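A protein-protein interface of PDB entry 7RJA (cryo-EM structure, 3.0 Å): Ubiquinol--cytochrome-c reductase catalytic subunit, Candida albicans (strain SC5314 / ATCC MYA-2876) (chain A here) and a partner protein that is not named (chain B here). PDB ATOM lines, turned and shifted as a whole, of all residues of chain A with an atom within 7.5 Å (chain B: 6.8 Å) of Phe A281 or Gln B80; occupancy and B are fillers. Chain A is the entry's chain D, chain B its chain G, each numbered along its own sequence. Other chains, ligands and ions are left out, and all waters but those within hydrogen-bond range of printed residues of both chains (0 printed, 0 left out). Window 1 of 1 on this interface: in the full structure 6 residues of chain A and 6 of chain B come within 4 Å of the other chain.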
ATOM      1  N   TRP A 273      28.142  -8.636  38.758  1.00  0.00           N
ATOM      2  CA  TRP A 273      28.049  -8.281  37.354  1.00  0.00           C
ATOM      3  C   TRP A 273      28.818  -9.222  36.445  1.00  0.00           C
ATOM      4  O   TRP A 273      28.665  -9.134  35.225  1.00  0.00           O
ATOM      5  CB  TRP A 273      28.559  -6.853  37.136  1.00  0.00           C
ATOM      6  CG  TRP A 273      27.504  -5.832  37.316  1.00  0.00           C
ATOM      7  CD1 TRP A 273      26.932  -5.441  38.484  1.00  0.00           C
ATOM      8  CD2 TRP A 273      26.883  -5.064  36.287  1.00  0.00           C
ATOM      9  NE1 TRP A 273      25.990  -4.474  38.249  1.00  0.00           N
ATOM     10  CE2 TRP A 273      25.944  -4.225  36.903  1.00  0.00           C
ATOM     11  CE3 TRP A 273      27.033  -5.004  34.902  1.00  0.00           C
ATOM     12  CZ2 TRP A 273      25.159  -3.338  36.185  1.00  0.00           C
ATOM     13  CZ3 TRP A 273      26.255  -4.125  34.192  1.00  0.00           C
ATOM     14  CH2 TRP A 273      25.329  -3.303  34.831  1.00  0.00           C
ATOM     15  N   THR A 274      29.642 -10.107  36.997  1.00  0.00           N
ATOM     16  CA  THR A 274      30.299 -11.105  36.160  1.00  0.00           C
ATOM     17  C   THR A 274      29.327 -11.858  35.259  1.00  0.00           C
ATOM     18  O   THR A 274      29.686 -12.118  34.099  1.00  0.00           O
ATOM     19  CB  THR A 274      31.093 -12.084  37.036  1.00  0.00           C
ATOM     20  OG1 THR A 274      30.333 -12.435  38.197  1.00  0.00           O
ATOM     21  CG2 THR A 274      32.408 -11.462  37.469  1.00  0.00           C
ATOM     22  N   PRO A 275      28.123 -12.241  35.696  1.00  0.00           N
ATOM     23  CA  PRO A 275      27.211 -12.908  34.755  1.00  0.00           C
ATOM     24  C   PRO A 275      26.843 -12.041  33.568  1.00  0.00           C
ATOM     25  O   PRO A 275      26.663 -12.561  32.462  1.00  0.00           O
ATOM     26  CB  PRO A 275      25.986 -13.226  35.624  1.00  0.00           C
ATOM     27  CG  PRO A 275      26.484 -13.161  37.018  1.00  0.00           C
ATOM     28  CD  PRO A 275      27.481 -12.059  37.004  1.00  0.00           C
ATOM     29  N   ILE A 276      26.722 -10.729  33.764  1.00  0.00           N
ATOM     30  CA  ILE A 276      26.294  -9.855  32.678  1.00  0.00           C
ATOM     31  C   ILE A 276      27.455  -9.537  31.752  1.00  0.00           C
ATOM     32  O   ILE A 276      27.324  -9.615  30.527  1.00  0.00           O
ATOM     33  CB  ILE A 276      25.662  -8.577  33.248  1.00  0.00           C
ATOM     34  CG1 ILE A 276      24.669  -8.920  34.354  1.00  0.00           C
ATOM     35  CG2 ILE A 276      24.967  -7.805  32.154  1.00  0.00           C
ATOM     36  CD1 ILE A 276      23.756 -10.074  34.023  1.00  0.00           C
ATOM     37  N   LYS A 277      28.607  -9.177  32.311  1.00  0.00           N
ATOM     38  CA  LYS A 277      29.768  -8.899  31.482  1.00  0.00           C
ATOM     39  C   LYS A 277      30.284 -10.144  30.774  1.00  0.00           C
ATOM     40  O   LYS A 277      31.093 -10.018  29.850  1.00  0.00           O
ATOM     41  CB  LYS A 277      30.872  -8.287  32.339  1.00  0.00           C
ATOM     42  CG  LYS A 277      30.507  -6.920  32.879  1.00  0.00           C
ATOM     43  CD  LYS A 277      31.722  -6.127  33.306  1.00  0.00           C
ATOM     44  CE  LYS A 277      31.331  -4.719  33.718  1.00  0.00           C
ATOM     45  NZ  LYS A 277      32.517  -3.885  34.044  1.00  0.00           N
ATOM     46  N   ASN A 278      29.837 -11.332  31.181  1.00  0.00           N
ATOM     47  CA  ASN A 278      30.220 -12.583  30.544  1.00  0.00           C
ATOM     48  C   ASN A 278      29.134 -13.137  29.636  1.00  0.00           C
ATOM     49  O   ASN A 278      29.246 -14.279  29.183  1.00  0.00           O
ATOM     50  CB  ASN A 278      30.580 -13.629  31.602  1.00  0.00           C
ATOM     51  CG  ASN A 278      31.785 -13.235  32.424  1.00  0.00           C
ATOM     52  OD1 ASN A 278      32.572 -12.379  32.023  1.00  0.00           O
ATOM     53  ND2 ASN A 278      31.937 -13.860  33.583  1.00  0.00           N
ATOM     54  N   ARG A 279      28.081 -12.373  29.365  1.00  0.00           N
ATOM     55  CA  ARG A 279      27.062 -12.836  28.438  1.00  0.00           C
ATOM     56  C   ARG A 279      27.649 -12.983  27.044  1.00  0.00           C
ATOM     57  O   ARG A 279      28.494 -12.197  26.613  1.00  0.00           O
ATOM     58  CB  ARG A 279      25.881 -11.869  28.393  1.00  0.00           C
ATOM     59  CG  ARG A 279      24.989 -11.930  29.606  1.00  0.00           C
ATOM     60  CD  ARG A 279      23.721 -11.127  29.404  1.00  0.00           C
ATOM     61  NE  ARG A 279      23.994  -9.756  28.995  1.00  0.00           N
ATOM     62  CZ  ARG A 279      23.061  -8.840  28.786  1.00  0.00           C
ATOM     63  NH1 ARG A 279      21.778  -9.110  28.953  1.00  0.00           N
ATOM     64  NH2 ARG A 279      23.423  -7.620  28.405  1.00  0.00           N
ATOM     65  N   LYS A 280      27.191 -14.008  26.334  1.00  0.00           N
ATOM     66  CA  LYS A 280      27.591 -14.226  24.954  1.00  0.00           C
ATOM     67  C   LYS A 280      26.350 -14.555  24.147  1.00  0.00           C
ATOM     68  O   LYS A 280      25.576 -15.438  24.525  1.00  0.00           O
ATOM     69  CB  LYS A 280      28.624 -15.349  24.845  1.00  0.00           C
ATOM     70  CG  LYS A 280      29.893 -15.051  25.611  1.00  0.00           C
ATOM     71  CD  LYS A 280      31.047 -15.915  25.160  1.00  0.00           C
ATOM     72  CE  LYS A 280      32.313 -15.537  25.894  1.00  0.00           C
ATOM     73  NZ  LYS A 280      32.749 -14.160  25.538  1.00  0.00           N
ATOM     74  N   PHE A 281      26.170 -13.846  23.043  1.00  0.00           N
ATOM     75  CA  PHE A 281      24.968 -13.937  22.233  1.00  0.00           C
ATOM     76  C   PHE A 281      25.246 -14.701  20.950  1.00  0.00           C
ATOM     77  O   PHE A 281      26.393 -14.836  20.520  1.00  0.00           O
ATOM     78  CB  PHE A 281      24.439 -12.551  21.870  1.00  0.00           C
ATOM     79  CG  PHE A 281      24.293 -11.637  23.032  1.00  0.00           C
ATOM     80  CD1 PHE A 281      23.439 -11.949  24.061  1.00  0.00           C
ATOM     81  CD2 PHE A 281      25.009 -10.466  23.098  1.00  0.00           C
ATOM     82  CE1 PHE A 281      23.296 -11.111  25.131  1.00  0.00           C
ATOM     83  CE2 PHE A 281      24.871  -9.629  24.164  1.00  0.00           C
ATOM     84  CZ  PHE A 281      24.013  -9.948  25.187  1.00  0.00           C
ATOM     85  N   ARG A 282      24.179 -15.203  20.350  1.00  0.00           N
ATOM     86  CA  ARG A 282      24.213 -15.686  18.983  1.00  0.00           C
ATOM     87  C   ARG A 282      22.956 -15.251  18.257  1.00  0.00           C
ATOM     88  O   ARG A 282      21.876 -15.188  18.848  1.00  0.00           O
ATOM     89  CB  ARG A 282      24.315 -17.185  18.886  1.00  0.00           C
ATOM     90  CG  ARG A 282      25.580 -17.798  19.402  1.00  0.00           C
ATOM     91  CD  ARG A 282      25.449 -19.277  19.211  1.00  0.00           C
ATOM     92  NE  ARG A 282      25.422 -19.557  17.778  1.00  0.00           N
ATOM     93  CZ  ARG A 282      24.355 -19.972  17.104  1.00  0.00           C
ATOM     94  NH1 ARG A 282      24.386 -20.139  15.794  1.00  0.00           N
ATOM     95  NH2 ARG A 282      23.237 -20.255  17.760  1.00  0.00           N
ATOM     96  N   PHE A 283      23.106 -14.949  16.974  1.00  0.00           N
ATOM     97  CA  PHE A 283      21.995 -14.601  16.100  1.00  0.00           C
ATOM     98  C   PHE A 283      22.112 -15.483  14.868  1.00  0.00           C
ATOM     99  O   PHE A 283      23.014 -15.289  14.048  1.00  0.00           O
ATOM    100  CB  PHE A 283      22.038 -13.121  15.743  1.00  0.00           C
ATOM    101  CG  PHE A 283      20.979 -12.696  14.782  1.00  0.00           C
ATOM    102  CD1 PHE A 283      19.648 -12.819  15.111  1.00  0.00           C
ATOM    103  CD2 PHE A 283      21.313 -12.139  13.563  1.00  0.00           C
ATOM    104  CE1 PHE A 283      18.670 -12.419  14.241  1.00  0.00           C
ATOM    105  CE2 PHE A 283      20.336 -11.735  12.688  1.00  0.00           C
ATOM    106  CZ  PHE A 283      19.012 -11.876  13.027  1.00  0.00           C
ATOM    107  N   MET B  41      31.051  -0.545  17.356  1.00  0.00           N
ATOM    108  CA  MET B  41      30.181  -1.254  18.280  1.00  0.00           C
ATOM    109  C   MET B  41      29.139  -2.097  17.562  1.00  0.00           C
ATOM    110  O   MET B  41      28.194  -2.572  18.198  1.00  0.00           O
ATOM    111  CB  MET B  41      29.492  -0.263  19.214  1.00  0.00           C
ATOM    112  CG  MET B  41      30.443   0.436  20.158  1.00  0.00           C
ATOM    113  SD  MET B  41      29.619   1.656  21.187  1.00  0.00           S
ATOM    114  CE  MET B  41      28.676   0.591  22.263  1.00  0.00           C
ATOM    115  N   PHE B  73      19.476  -7.686  17.075  1.00  0.00           N
ATOM    116  CA  PHE B  73      20.750  -8.268  17.477  1.00  0.00           C
ATOM    117  C   PHE B  73      21.852  -7.222  17.512  1.00  0.00           C
ATOM    118  O   PHE B  73      22.694  -7.239  18.413  1.00  0.00           O
ATOM    119  CB  PHE B  73      21.143  -9.407  16.547  1.00  0.00           C
ATOM    120  CG  PHE B  73      22.477  -9.998  16.870  1.00  0.00           C
ATOM    121  CD1 PHE B  73      22.691 -10.624  18.083  1.00  0.00           C
ATOM    122  CD2 PHE B  73      23.519  -9.926  15.968  1.00  0.00           C
ATOM    123  CE1 PHE B  73      23.912 -11.170  18.387  1.00  0.00           C
ATOM    124  CE2 PHE B  73      24.745 -10.471  16.269  1.00  0.00           C
ATOM    125  CZ  PHE B  73      24.941 -11.093  17.482  1.00  0.00           C
ATOM    126  N   ILE B  75      21.527  -3.983  18.081  1.00  0.00           N
ATOM    127  CA  ILE B  75      21.312  -3.136  19.249  1.00  0.00           C
ATOM    128  C   ILE B  75      21.741  -3.862  20.515  1.00  0.00           C
ATOM    129  O   ILE B  75      22.368  -3.275  21.404  1.00  0.00           O
ATOM    130  CB  ILE B  75      19.841  -2.693  19.325  1.00  0.00           C
ATOM    131  CG1 ILE B  75      19.552  -1.663  18.234  1.00  0.00           C
ATOM    132  CG2 ILE B  75      19.534  -2.140  20.706  1.00  0.00           C
ATOM    133  CD1 ILE B  75      18.098  -1.292  18.109  1.00  0.00           C
ATOM    134  N   LEU B  76      21.400  -5.145  20.630  1.00  0.00           N
ATOM    135  CA  LEU B  76      21.807  -5.905  21.806  1.00  0.00           C
ATOM    136  C   LEU B  76      23.324  -6.008  21.894  1.00  0.00           C
ATOM    137  O   LEU B  76      23.899  -5.894  22.982  1.00  0.00           O
ATOM    138  CB  LEU B  76      21.173  -7.291  21.772  1.00  0.00           C
ATOM    139  CG  LEU B  76      21.645  -8.257  22.853  1.00  0.00           C
ATOM    140  CD1 LEU B  76      21.316  -7.714  24.221  1.00  0.00           C
ATOM    141  CD2 LEU B  76      21.004  -9.611  22.649  1.00  0.00           C
ATOM    142  N   THR B  77      23.988  -6.232  20.761  1.00  0.00           N
ATOM    143  CA  THR B  77      25.444  -6.300  20.759  1.00  0.00           C
ATOM    144  C   THR B  77      26.052  -4.970  21.175  1.00  0.00           C
ATOM    145  O   THR B  77      27.040  -4.937  21.915  1.00  0.00           O
ATOM    146  CB  THR B  77      25.947  -6.706  19.377  1.00  0.00           C
ATOM    147  OG1 THR B  77      25.598  -8.070  19.124  1.00  0.00           O
ATOM    148  CG2 THR B  77      27.451  -6.549  19.290  1.00  0.00           C
ATOM    149  N   ALA B  78      25.487  -3.863  20.697  1.00  0.00           N
ATOM    150  CA  ALA B  78      25.989  -2.553  21.097  1.00  0.00           C
ATOM    151  C   ALA B  78      25.809  -2.333  22.589  1.00  0.00           C
ATOM    152  O   ALA B  78      26.706  -1.809  23.262  1.00  0.00           O
ATOM    153  CB  ALA B  78      25.278  -1.459  20.309  1.00  0.00           C
ATOM    154  N   HIS B  79      24.654  -2.718  23.128  1.00  0.00           N
ATOM    155  CA  HIS B  79      24.441  -2.593  24.564  1.00  0.00           C
ATOM    156  C   HIS B  79      25.458  -3.412  25.338  1.00  0.00           C
ATOM    157  O   HIS B  79      26.024  -2.936  26.325  1.00  0.00           O
ATOM    158  CB  HIS B  79      23.029  -3.033  24.935  1.00  0.00           C
ATOM    159  CG  HIS B  79      22.016  -1.939  24.844  1.00  0.00           C
ATOM    160  ND1 HIS B  79      21.547  -1.456  23.642  1.00  0.00           N
ATOM    161  CD2 HIS B  79      21.386  -1.228  25.807  1.00  0.00           C
ATOM    162  CE1 HIS B  79      20.668  -0.498  23.870  1.00  0.00           C
ATOM    163  NE2 HIS B  79      20.553  -0.339  25.175  1.00  0.00           N
ATOM    164  N   GLN B  80      25.707  -4.645  24.904  1.00  0.00           N
ATOM    165  CA  GLN B  80      26.675  -5.487  25.597  1.00  0.00           C
ATOM    166  C   GLN B  80      28.079  -4.901  25.520  1.00  0.00           C
ATOM    167  O   GLN B  80      28.829  -4.936  26.500  1.00  0.00           O
ATOM    168  CB  GLN B  80      26.648  -6.892  25.011  1.00  0.00           C
ATOM    169  CG  GLN B  80      27.631  -7.854  25.636  1.00  0.00           C
ATOM    170  CD  GLN B  80      27.399  -8.041  27.111  1.00  0.00           C
ATOM    171  OE1 GLN B  80      26.317  -7.760  27.619  1.00  0.00           O
ATOM    172  NE2 GLN B  80      28.413  -8.524  27.812  1.00  0.00           N
ATOM    173  N   LEU B  81      28.461  -4.376  24.358  1.00  0.00           N
ATOM    174  CA  LEU B  81      29.794  -3.802  24.220  1.00  0.00           C
ATOM    175  C   LEU B  81      29.958  -2.577  25.108  1.00  0.00           C
ATOM    176  O   LEU B  81      30.990  -2.416  25.765  1.00  0.00           O
ATOM    177  CB  LEU B  81      30.059  -3.451  22.762  1.00  0.00           C
ATOM    178  CG  LEU B  81      30.203  -4.659  21.842  1.00  0.00           C
ATOM    179  CD1 LEU B  81      30.257  -4.214  20.404  1.00  0.00           C
ATOM    180  CD2 LEU B  81      31.438  -5.457  22.196  1.00  0.00           C
ATOM    181  N   ALA B  82      28.953  -1.701  25.143  1.00  0.00           N
ATOM    182  CA  ALA B  82      29.012  -0.573  26.064  1.00  0.00           C
ATOM    183  C   ALA B  82      29.035  -1.046  27.506  1.00  0.00           C
ATOM    184  O   ALA B  82      29.685  -0.429  28.355  1.00  0.00           O
ATOM    185  CB  ALA B  82      27.823   0.357  25.837  1.00  0.00           C
ATOM    186  N   LEU B  83      28.329  -2.136  27.801  1.00  0.00           N
ATOM    187  CA  LEU B  83      28.283  -2.668  29.155  1.00  0.00           C
ATOM    188  C   LEU B  83      29.648  -3.167  29.602  1.00  0.00           C
ATOM    189  O   LEU B  83      30.053  -2.939  30.746  1.00  0.00           O
ATOM    190  CB  LEU B  83      27.255  -3.797  29.206  1.00  0.00           C
ATOM    191  CG  LEU B  83      26.883  -4.410  30.550  1.00  0.00           C
ATOM    192  CD1 LEU B  83      25.482  -4.981  30.484  1.00  0.00           C
ATOM    193  CD2 LEU B  83      27.863  -5.489  30.935  1.00  0.00           C
ATOM    194  N   SER B  84      30.368  -3.850  28.717  1.00  0.00           N
ATOM    195  CA  SER B  84      31.657  -4.438  29.044  1.00  0.00           C
ATOM    196  C   SER B  84      32.830  -3.548  28.657  1.00  0.00           C
ATOM    197  O   SER B  84      33.981  -3.971  28.783  1.00  0.00           O
ATOM    198  CB  SER B  84      31.793  -5.802  28.370  1.00  0.00           C
ATOM    199  OG  SER B  84      31.595  -5.698  26.974  1.00  0.00           O
ATOM    200  N   HIS B  85      32.568  -2.330  28.191  1.00  0.00           N
ATOM    201  CA  HIS B  85      33.623  -1.369  27.883  1.00  0.00           C
ATOM    202  C   HIS B  85      34.657  -1.968  26.938  1.00  0.00           C
ATOM    203  O   HIS B  85      35.866  -1.867  27.155  1.00  0.00           O
ATOM    204  CB  HIS B  85      34.289  -0.870  29.163  1.00  0.00           C
ATOM    205  CG  HIS B  85      33.373  -0.104  30.060  1.00  0.00           C
ATOM    206  ND1 HIS B  85      33.140  -0.466  31.369  1.00  0.00           N
ATOM    207  CD2 HIS B  85      32.635   1.009  29.840  1.00  0.00           C
ATOM    208  CE1 HIS B  85      32.295   0.388  31.915  1.00  0.00           C
ATOM    209  NE2 HIS B  85      31.974   1.294  31.009  1.00  0.00           N
ATOM    210  N   GLN B  86      34.175  -2.604  25.876  1.00  0.00           N
ATOM    211  CA  GLN B  86      35.064  -3.146  24.863  1.00  0.00           C
ATOM    212  C   GLN B  86      34.434  -2.937  23.496  1.00  0.00           C
ATOM    213  O   GLN B  86      33.218  -2.786  23.367  1.00  0.00           O
ATOM    214  CB  GLN B  86      35.361  -4.629  25.106  1.00  0.00           C
ATOM    215  CG  GLN B  86      34.158  -5.530  24.980  1.00  0.00           C
ATOM    216  CD  GLN B  86      34.465  -6.957  25.373  1.00  0.00           C
ATOM    217  OE1 GLN B  86      35.600  -7.286  25.713  1.00  0.00           O
ATOM    218  NE2 GLN B  86      33.453  -7.815  25.327  1.00  0.00           N
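Among the printed residues, pairs that only touch across the chains: Trp A273 with Leu B83 (3.7 Å), Ile A276 with Leu B83 (3.3 Å), Lys A277 with Gln B80 (3.7 Å), Lys A277 with Leu B83 (3.6 Å), Arg A279 with Leu B83 (3.9 Å), Phe A281 with Phe B73 (3.8 Å), Phe A281 with Leu B76 (3.6 Å), Phe A281 with Gln B80 (3.4 Å) and Phe A283 with Phe B73 (3.3 Å).
The backbone carbonyl oxygen of Phe B73 lies within hydrogen-bond range of the side-chain hydroxyl of Thr B77 (3.1 Å). The backbone carbonyl oxygen of Gln B80 lies within hydrogen-bond range of the side-chain hydroxyl of Ser B84.
NE2 of Gln B80 lies within hydrogen-bond range of O of Ile A276 (3.1 Å). The guanidinium group (NH2) of Arg A279 sits at hydrogen-bond distance from the side-chain amide oxygen (OE1) of Gln B80 (3.0 Å).
Printed residues of chain A that touch a printed residue of chain B: Trp A273, Ile A276, Lys A277, Arg A279, Phe A281 and Phe A283. Of the 14 printed residues of chain B, 4 touch a printed residue of chain A. Hydrophobic or aromatic side chains of chain B within 4 Å of the printed part of chain A: Phe B73, Leu B76 and Leu B83. Among the printed residues, 11 pairs touch across the chains.
Of chain B, only Phe B73 (3.8 Å), Leu B76 (3.6 Å) and Gln B80 (3.4 Å) come within 4 Å of Phe A281. Of chain A, only Ile A276, Lys A277, Arg A279 and Phe A281 come within 4 Å of Gln B80. Printed residues of chain A within 4 Å of Leu B76: Phe A281 (3.6 Å). Of the printed residues of chain B, Lys A277 touches Gln B80 (3.7 Å) and Leu B83 (3.6 Å). Of the printed residues of chain B, Ile A276 touches Gln B80 (3.1 Å) and Leu B83 (3.3 Å). Of the printed residues of chain B, Arg A279 touches Gln B80 (3.0 Å) and Leu B83 (3.9 Å). Of the printed residues of chain B, Phe A283 touches Phe B73 (3.3 Å). Leu B81 touches none of the printed residues of chain A. His B85 touches none of the printed residues of chain A. The nearest residue of chain A that does not touch Gln B80 is Asn A278 (4.6 Å).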
